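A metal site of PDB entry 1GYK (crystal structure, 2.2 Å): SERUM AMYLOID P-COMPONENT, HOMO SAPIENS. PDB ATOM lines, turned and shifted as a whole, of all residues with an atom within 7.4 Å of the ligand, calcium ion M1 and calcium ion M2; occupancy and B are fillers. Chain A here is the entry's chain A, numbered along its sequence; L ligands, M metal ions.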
ATOM      1  N   SER A  48      29.443   0.677   0.703  1.00  0.00           N
ATOM      2  CA  SER A  48      28.744   1.076  -0.506  1.00  0.00           C
ATOM      3  C   SER A  48      29.732   1.745  -1.469  1.00  0.00           C
ATOM      4  O   SER A  48      30.656   2.467  -1.040  1.00  0.00           O
ATOM      5  CB  SER A  48      27.602   1.986  -0.130  1.00  0.00           C
ATOM      6  OG  SER A  48      26.898   2.555  -1.199  1.00  0.00           O
ATOM      7  N   SER A  51      25.462   4.586  -4.571  1.00  0.00           N
ATOM      8  CA  SER A  51      24.124   4.671  -3.962  1.00  0.00           C
ATOM      9  C   SER A  51      23.260   5.615  -4.794  1.00  0.00           C
ATOM     10  O   SER A  51      23.576   6.772  -4.948  1.00  0.00           O
ATOM     11  CB  SER A  51      24.200   5.124  -2.490  1.00  0.00           C
ATOM     12  OG  SER A  51      22.945   5.195  -1.844  1.00  0.00           O
ATOM     13  N   TYR A  52      22.148   5.075  -5.294  1.00  0.00           N
ATOM     14  CA  TYR A  52      21.147   5.765  -6.121  1.00  0.00           C
ATOM     15  C   TYR A  52      19.835   5.335  -5.445  1.00  0.00           C
ATOM     16  O   TYR A  52      19.511   4.135  -5.337  1.00  0.00           O
ATOM     17  CB  TYR A  52      21.320   5.255  -7.583  1.00  0.00           C
ATOM     18  CG  TYR A  52      20.423   5.656  -8.762  1.00  0.00           C
ATOM     19  CD1 TYR A  52      18.986   5.447  -8.780  1.00  0.00           C
ATOM     20  CD2 TYR A  52      21.049   6.083 -10.000  1.00  0.00           C
ATOM     21  CE1 TYR A  52      18.195   5.644  -9.987  1.00  0.00           C
ATOM     22  CE2 TYR A  52      20.260   6.277 -11.231  1.00  0.00           C
ATOM     23  CZ  TYR A  52      18.843   6.048 -11.200  1.00  0.00           C
ATOM     24  OH  TYR A  52      18.121   6.252 -12.344  1.00  0.00           O
ATOM     25  N   ASN A  53      19.116   6.369  -5.002  1.00  0.00           N
ATOM     26  CA  ASN A  53      17.797   6.296  -4.351  1.00  0.00           C
ATOM     27  C   ASN A  53      16.863   7.309  -4.999  1.00  0.00           C
ATOM     28  O   ASN A  53      17.290   8.406  -5.372  1.00  0.00           O
ATOM     29  CB  ASN A  53      17.876   6.680  -2.858  1.00  0.00           C
ATOM     30  CG  ASN A  53      18.353   5.553  -1.943  1.00  0.00           C
ATOM     31  OD1 ASN A  53      18.990   4.581  -2.368  1.00  0.00           O
ATOM     32  ND2 ASN A  53      17.992   5.660  -0.660  1.00  0.00           N
ATOM     33  N   ASP A  58      14.319   3.368  -1.639  1.00  0.00           N
ATOM     34  CA  ASP A  58      15.648   2.997  -1.110  1.00  0.00           C
ATOM     35  C   ASP A  58      16.187   1.773  -1.833  1.00  0.00           C
ATOM     36  O   ASP A  58      15.439   0.836  -2.018  1.00  0.00           O
ATOM     37  CB  ASP A  58      15.576   2.727   0.433  1.00  0.00           C
ATOM     38  CG  ASP A  58      16.954   2.397   1.076  1.00  0.00           C
ATOM     39  OD1 ASP A  58      17.958   3.045   0.736  1.00  0.00           O
ATOM     40  OD2 ASP A  58      17.028   1.442   1.876  1.00  0.00           O
ATOM     41  N   ASN A  59      17.503   1.757  -2.114  1.00  0.00           N
ATOM     42  CA  ASN A  59      18.281   0.660  -2.805  1.00  0.00           C
ATOM     43  C   ASN A  59      17.774   0.360  -4.211  1.00  0.00           C
ATOM     44  O   ASN A  59      17.633  -0.814  -4.631  1.00  0.00           O
ATOM     45  CB  ASN A  59      18.381  -0.646  -1.955  1.00  0.00           C
ATOM     46  CG  ASN A  59      18.917  -0.424  -0.553  1.00  0.00           C
ATOM     47  OD1 ASN A  59      19.409   0.670  -0.185  1.00  0.00           O
ATOM     48  ND2 ASN A  59      18.863  -1.491   0.242  1.00  0.00           N
ATOM     49  N   GLU A  60      17.454   1.466  -4.908  1.00  0.00           N
ATOM     50  CA  GLU A  60      16.932   1.460  -6.274  1.00  0.00           C
ATOM     51  C   GLU A  60      17.992   0.974  -7.276  1.00  0.00           C
ATOM     52  O   GLU A  60      17.670   0.209  -8.200  1.00  0.00           O
ATOM     53  CB  GLU A  60      16.355   2.863  -6.613  1.00  0.00           C
ATOM     54  CG  GLU A  60      15.654   3.078  -8.030  1.00  0.00           C
ATOM     55  CD  GLU A  60      14.375   2.264  -8.297  1.00  0.00           C
ATOM     56  OE1 GLU A  60      13.931   1.438  -7.523  1.00  0.00           O
ATOM     57  OE2 GLU A  60      13.763   2.480  -9.331  1.00  0.00           O
ATOM     58  N   LEU A  62      22.054   0.082  -6.232  1.00  0.00           N
ATOM     59  CA  LEU A  62      23.168   0.036  -5.299  1.00  0.00           C
ATOM     60  C   LEU A  62      24.264  -0.997  -5.618  1.00  0.00           C
ATOM     61  O   LEU A  62      23.980  -2.181  -5.710  1.00  0.00           O
ATOM     62  CB  LEU A  62      22.674  -0.090  -3.832  1.00  0.00           C
ATOM     63  CG  LEU A  62      23.589  -0.338  -2.618  1.00  0.00           C
ATOM     64  CD1 LEU A  62      24.405   0.889  -2.315  1.00  0.00           C
ATOM     65  CD2 LEU A  62      22.782  -0.708  -1.451  1.00  0.00           C
ATOM     66  N   TYR A  64      27.324  -2.586  -3.918  1.00  0.00           N
ATOM     67  CA  TYR A  64      27.742  -2.877  -2.560  1.00  0.00           C
ATOM     68  C   TYR A  64      28.799  -3.959  -2.487  1.00  0.00           C
ATOM     69  O   TYR A  64      28.659  -4.974  -3.155  1.00  0.00           O
ATOM     70  CB  TYR A  64      26.482  -3.346  -1.788  1.00  0.00           C
ATOM     71  CG  TYR A  64      26.522  -3.252  -0.278  1.00  0.00           C
ATOM     72  CD1 TYR A  64      26.459  -1.970   0.381  1.00  0.00           C
ATOM     73  CD2 TYR A  64      26.615  -4.441   0.532  1.00  0.00           C
ATOM     74  CE1 TYR A  64      26.488  -1.854   1.847  1.00  0.00           C
ATOM     75  CE2 TYR A  64      26.620  -4.343   2.002  1.00  0.00           C
ATOM     76  CZ  TYR A  64      26.560  -3.051   2.631  1.00  0.00           C
ATOM     77  OH  TYR A  64      26.528  -2.920   3.999  1.00  0.00           O
ATOM     78  N   GLU A  66      30.357  -6.728  -0.168  1.00  0.00           N
ATOM     79  CA  GLU A  66      30.050  -7.514   1.042  1.00  0.00           C
ATOM     80  C   GLU A  66      31.246  -7.781   1.951  1.00  0.00           C
ATOM     81  O   GLU A  66      31.175  -7.627   3.177  1.00  0.00           O
ATOM     82  CB  GLU A  66      29.413  -8.863   0.674  1.00  0.00           C
ATOM     83  CG  GLU A  66      28.112  -8.821  -0.166  1.00  0.00           C
ATOM     84  CD  GLU A  66      26.881  -8.201   0.549  1.00  0.00           C
ATOM     85  OE1 GLU A  66      26.779  -8.245   1.809  1.00  0.00           O
ATOM     86  OE2 GLU A  66      26.013  -7.663  -0.175  1.00  0.00           O
ATOM     87  N   TYR A  74      22.042  -4.181  -6.302  1.00  0.00           N
ATOM     88  CA  TYR A  74      20.668  -4.019  -5.908  1.00  0.00           C
ATOM     89  C   TYR A  74      19.930  -3.271  -6.994  1.00  0.00           C
ATOM     90  O   TYR A  74      20.445  -2.302  -7.517  1.00  0.00           O
ATOM     91  CB  TYR A  74      20.524  -3.242  -4.610  1.00  0.00           C
ATOM     92  CG  TYR A  74      20.953  -3.909  -3.340  1.00  0.00           C
ATOM     93  CD1 TYR A  74      22.354  -4.105  -3.025  1.00  0.00           C
ATOM     94  CD2 TYR A  74      19.969  -4.286  -2.351  1.00  0.00           C
ATOM     95  CE1 TYR A  74      22.767  -4.652  -1.739  1.00  0.00           C
ATOM     96  CE2 TYR A  74      20.365  -4.841  -1.052  1.00  0.00           C
ATOM     97  CZ  TYR A  74      21.759  -5.018  -0.770  1.00  0.00           C
ATOM     98  OH  TYR A  74      22.098  -5.560   0.444  1.00  0.00           O
ATOM     99  N   ARG A  77      15.313  -2.860  -4.410  1.00  0.00           N
ATOM    100  CA  ARG A  77      15.295  -3.634  -3.104  1.00  0.00           C
ATOM    101  C   ARG A  77      15.820  -5.066  -3.212  1.00  0.00           C
ATOM    102  O   ARG A  77      16.221  -5.658  -2.214  1.00  0.00           O
ATOM    103  CB  ARG A  77      13.928  -3.675  -2.346  1.00  0.00           C
ATOM    104  CG  ARG A  77      13.456  -2.371  -1.735  1.00  0.00           C
ATOM    105  CD  ARG A  77      11.943  -2.128  -1.932  1.00  0.00           C
ATOM    106  NE  ARG A  77      11.468  -2.062  -3.328  1.00  0.00           N
ATOM    107  CZ  ARG A  77      11.148  -0.939  -4.007  1.00  0.00           C
ATOM    108  NH1 ARG A  77      11.246   0.276  -3.471  1.00  0.00           N
ATOM    109  NH2 ARG A  77      10.735  -1.038  -5.270  1.00  0.00           N
ATOM    110  N   LYS A  79      18.460  -7.945  -4.404  1.00  0.00           N
ATOM    111  CA  LYS A  79      19.912  -8.099  -4.587  1.00  0.00           C
ATOM    112  C   LYS A  79      20.342  -9.326  -5.380  1.00  0.00           C
ATOM    113  O   LYS A  79      19.572 -10.297  -5.542  1.00  0.00           O
ATOM    114  CB  LYS A  79      20.684  -7.965  -3.254  1.00  0.00           C
ATOM    115  CG  LYS A  79      20.559  -9.109  -2.216  1.00  0.00           C
ATOM    116  CD  LYS A  79      21.236  -8.797  -0.872  1.00  0.00           C
ATOM    117  CE  LYS A  79      22.766  -8.766  -0.902  1.00  0.00           C
ATOM    118  NZ  LYS A  79      23.344  -8.364   0.427  1.00  0.00           N
ATOM    119  N   GLU A 136      26.106   5.418   1.898  1.00  0.00           N
ATOM    120  CA  GLU A 136      24.914   4.602   1.554  1.00  0.00           C
ATOM    121  C   GLU A 136      23.702   5.410   2.045  1.00  0.00           C
ATOM    122  O   GLU A 136      23.590   5.711   3.249  1.00  0.00           O
ATOM    123  CB  GLU A 136      24.929   3.257   2.332  1.00  0.00           C
ATOM    124  CG  GLU A 136      24.202   2.042   1.696  1.00  0.00           C
ATOM    125  CD  GLU A 136      22.692   2.111   1.658  1.00  0.00           C
ATOM    126  OE1 GLU A 136      22.064   2.263   2.736  1.00  0.00           O
ATOM    127  OE2 GLU A 136      22.155   2.094   0.531  1.00  0.00           O
ATOM    128  N   GLN A 137      22.729   5.591   1.156  1.00  0.00           N
ATOM    129  CA  GLN A 137      21.509   6.328   1.481  1.00  0.00           C
ATOM    130  C   GLN A 137      20.384   5.405   1.945  1.00  0.00           C
ATOM    131  O   GLN A 137      20.266   4.318   1.392  1.00  0.00           O
ATOM    132  CB  GLN A 137      20.962   7.090   0.272  1.00  0.00           C
ATOM    133  CG  GLN A 137      21.849   8.076  -0.433  1.00  0.00           C
ATOM    134  CD  GLN A 137      21.280   8.441  -1.792  1.00  0.00           C
ATOM    135  OE1 GLN A 137      20.420   9.303  -1.912  1.00  0.00           O
ATOM    136  NE2 GLN A 137      21.762   7.774  -2.821  1.00  0.00           N
ATOM    137  N   ASP A 138      19.668   5.818   3.012  1.00  0.00           N
ATOM    138  CA  ASP A 138      18.472   5.100   3.523  1.00  0.00           C
ATOM    139  C   ASP A 138      17.214   5.987   3.422  1.00  0.00           C
ATOM    140  O   ASP A 138      16.168   5.708   4.034  1.00  0.00           O
ATOM    141  CB  ASP A 138      18.645   4.466   4.926  1.00  0.00           C
ATOM    142  CG  ASP A 138      19.467   3.162   4.929  1.00  0.00           C
ATOM    143  OD1 ASP A 138      19.507   2.385   3.948  1.00  0.00           O
ATOM    144  OD2 ASP A 138      20.055   2.900   5.991  1.00  0.00           O
ATOM    145  N   SER A 139      17.358   7.062   2.629  1.00  0.00           N
ATOM    146  CA  SER A 139      16.315   8.041   2.270  1.00  0.00           C
ATOM    147  C   SER A 139      16.765   8.747   0.970  1.00  0.00           C
ATOM    148  O   SER A 139      17.758   8.317   0.340  1.00  0.00           O
ATOM    149  CB  SER A 139      16.052   9.043   3.406  1.00  0.00           C
ATOM    150  OG  SER A 139      17.090   9.977   3.561  1.00  0.00           O
ATOM    151  N   GLY A 142      19.845  11.310   2.111  1.00  0.00           N
ATOM    152  CA  GLY A 142      20.377  11.225   3.468  1.00  0.00           C
ATOM    153  C   GLY A 142      20.249   9.878   4.111  1.00  0.00           C
ATOM    154  O   GLY A 142      20.194   8.859   3.414  1.00  0.00           O
ATOM    155  N   LYS A 143      20.102   9.908   5.449  1.00  0.00           N
ATOM    156  CA  LYS A 143      19.988   8.739   6.364  1.00  0.00           C
ATOM    157  C   LYS A 143      21.159   7.698   6.201  1.00  0.00           C
ATOM    158  O   LYS A 143      21.004   6.531   5.787  1.00  0.00           O
ATOM    159  CB  LYS A 143      18.584   8.101   6.307  1.00  0.00           C
ATOM    160  CG  LYS A 143      17.551   8.747   7.220  1.00  0.00           C
ATOM    161  CD  LYS A 143      16.204   7.996   7.195  1.00  0.00           C
ATOM    162  CE  LYS A 143      16.186   6.680   7.991  1.00  0.00           C
ATOM    163  NZ  LYS A 143      16.417   6.905   9.451  1.00  0.00           N
ATOM    164  N   PHE A 144      22.360   8.230   6.432  1.00  0.00           N
ATOM    165  CA  PHE A 144      23.602   7.494   6.298  1.00  0.00           C
ATOM    166  C   PHE A 144      23.955   6.645   7.515  1.00  0.00           C
ATOM    167  O   PHE A 144      23.424   6.875   8.616  1.00  0.00           O
ATOM    168  CB  PHE A 144      24.752   8.463   5.950  1.00  0.00           C
ATOM    169  CG  PHE A 144      24.480   9.395   4.762  1.00  0.00           C
ATOM    170  CD1 PHE A 144      23.857   8.940   3.544  1.00  0.00           C
ATOM    171  CD2 PHE A 144      24.953  10.735   4.825  1.00  0.00           C
ATOM    172  CE1 PHE A 144      23.743   9.808   2.364  1.00  0.00           C
ATOM    173  CE2 PHE A 144      24.860  11.633   3.668  1.00  0.00           C
ATOM    174  CZ  PHE A 144      24.241  11.165   2.423  1.00  0.00           C
ATOM    175  N   ASP A 145      24.877   5.711   7.277  1.00  0.00           N
ATOM    176  CA  ASP A 145      25.395   4.764   8.264  1.00  0.00           C
ATOM    177  C   ASP A 145      26.927   4.696   8.135  1.00  0.00           C
ATOM    178  O   ASP A 145      27.448   4.275   7.094  1.00  0.00           O
ATOM    179  CB  ASP A 145      24.712   3.383   8.003  1.00  0.00           C
ATOM    180  CG  ASP A 145      24.949   2.332   9.100  1.00  0.00           C
ATOM    181  OD1 ASP A 145      25.657   2.554  10.123  1.00  0.00           O
ATOM    182  OD2 ASP A 145      24.440   1.224   8.910  1.00  0.00           O
ATOM    183  N   SER A 147      29.012   2.476   9.345  1.00  0.00           N
ATOM    184  CA  SER A 147      29.414   1.080   9.103  1.00  0.00           C
ATOM    185  C   SER A 147      29.383   0.657   7.631  1.00  0.00           C
ATOM    186  O   SER A 147      29.945  -0.386   7.246  1.00  0.00           O
ATOM    187  CB  SER A 147      28.556   0.130   9.959  1.00  0.00           C
ATOM    188  OG  SER A 147      27.207   0.056   9.514  1.00  0.00           O
ATOM    189  N   GLN A 148      28.652   1.447   6.841  1.00  0.00           N
ATOM    190  CA  GLN A 148      28.495   1.251   5.409  1.00  0.00           C
ATOM    191  C   GLN A 148      29.287   2.312   4.599  1.00  0.00           C
ATOM    192  O   GLN A 148      29.252   2.275   3.367  1.00  0.00           O
ATOM    193  CB  GLN A 148      27.022   1.300   5.033  1.00  0.00           C
ATOM    194  CG  GLN A 148      26.133   0.251   5.664  1.00  0.00           C
ATOM    195  CD  GLN A 148      24.747   0.282   5.087  1.00  0.00           C
ATOM    196  OE1 GLN A 148      24.093   1.351   5.028  1.00  0.00           O
ATOM    197  NE2 GLN A 148      24.240  -0.892   4.691  1.00  0.00           N
HETATM  198  C1  LIG L   1      20.448  -6.171   5.367  1.00  0.00           C
HETATM  199  C2  LIG L   1      20.396  -3.200   5.331  1.00  0.00           C
HETATM  200  C3  LIG L   1      19.340  -4.072   4.593  1.00  0.00           C
HETATM  201  C4  LIG L   1      18.932  -3.318   3.297  1.00  0.00           C
HETATM  202  C5  LIG L   1      21.294  -2.375   3.090  1.00  0.00           C
HETATM  203  C6  LIG L   1      20.921  -0.850   3.351  1.00  0.00           C
HETATM  204  C7  LIG L   1      22.470  -2.221   2.170  1.00  0.00           C
HETATM  205  O1  LIG L   1      21.804  -6.091   7.414  1.00  0.00           O
HETATM  206  O2  LIG L   1      21.877  -3.141   7.254  1.00  0.00           O
HETATM  207  O3  LIG L   1      21.549  -2.944   4.441  1.00  0.00           O
HETATM  208  O4  LIG L   1      20.097  -3.001   2.463  1.00  0.00           O
HETATM  209  O5  LIG L   1      21.319  -0.299   4.407  1.00  0.00           O
HETATM  210  O6  LIG L   1      20.191  -0.243   2.535  1.00  0.00           O
HETATM  211 CA    CA M   1      21.988   1.894   4.968  1.00  0.00          CA
HETATM  212 CA    CA M   2      19.802   2.003   1.535  1.00  0.00          CA
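Residues that only touch the ligand: Leu 62 (3.9 Å) and Tyr 74 (3.8 Å). Hydrophobic or aromatic side chains within 4 Å of the ligand: Leu 62 and Tyr 74. Of the 23 residues printed, 7 come within 4 Å of the ligand. The nearest printed residue that does not touch the ligand is Tyr 64 (4.05 Å).
Five residues have an atom within 4 Å of calcium ion M2: Asp 58, Asn 59, Glu 136, Gln 137 and Asp 138. The nearest printed residue that does not touch calcium ion M2 is Asn 53 (4.6 Å).
Of the 23 residues printed, 3 come within 4 Å of calcium ion M1. The nearest printed residue that does not touch calcium ion M1 is Asp 145 (4.3 Å).
Calcium ion M2 is bound by the side-chain amide oxygen (OD1) of Asn 59, the side-chain carboxylate (OD1) of Asp 58, the backbone carbonyl oxygen (O) of Gln 137, the side-chain carboxylate (OD1) of Asp 138, an oxygen (O6) of the ligand, the side-chain carboxylate (OE2) of Glu 136, the side-chain carboxylate (OE1) of Glu 136 and the side-chain carboxylate (OD2) of Asp 58.
NE2 of Gln 148 sits at hydrogen-bond distance from OH of Tyr 64, 3.1 Å away. The backbone carbonyl oxygen (O) of Gln 148 sits at hydrogen-bond distance from the backbone NH (N) of Ser 48, at 3.1 Å. The backbone NH of Asn 59 is in hydrogen-bond range of the side-chain amide oxygen of Asn 53 (3.2 Å). N of Arg 77 is in hydrogen-bond range of O of Asn 59 (3.1 Å). The side-chain amide nitrogen (ND2) of Asn 53 sits close to the backbone carbonyl oxygen (O) of Gln 137, at 3.3 Å. NE2 of Gln 137 is in hydrogen-bond range of O of Ser 51 (3.0 Å). The backbone carbonyl oxygen (O) of Lys 143 sits at hydrogen-bond distance from the backbone NH (N) of Asp 138 (3.2 Å). The backbone NH of Tyr 74 lies within hydrogen-bond range of the backbone carbonyl oxygen of Leu 62 (2.8 Å).
OE1 of Gln 148 binds calcium ion M1 (2.2 Å). Calcium ion M1 is bound by the side-chain carboxylate (OE1) of Glu 136 (2.3 Å). An oxygen (O5) of the ligand binds calcium ion M1, 2.4 Å away. The side-chain carboxylate (OD2) of Asp 138 is bound to calcium ion M1 (2.4 Å). Calcium ion M1 is bound by the side-chain carboxylate (OD1) of Asp 138, 2.7 Å away. Calcium ion M1 has five donor atoms within binding distance.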
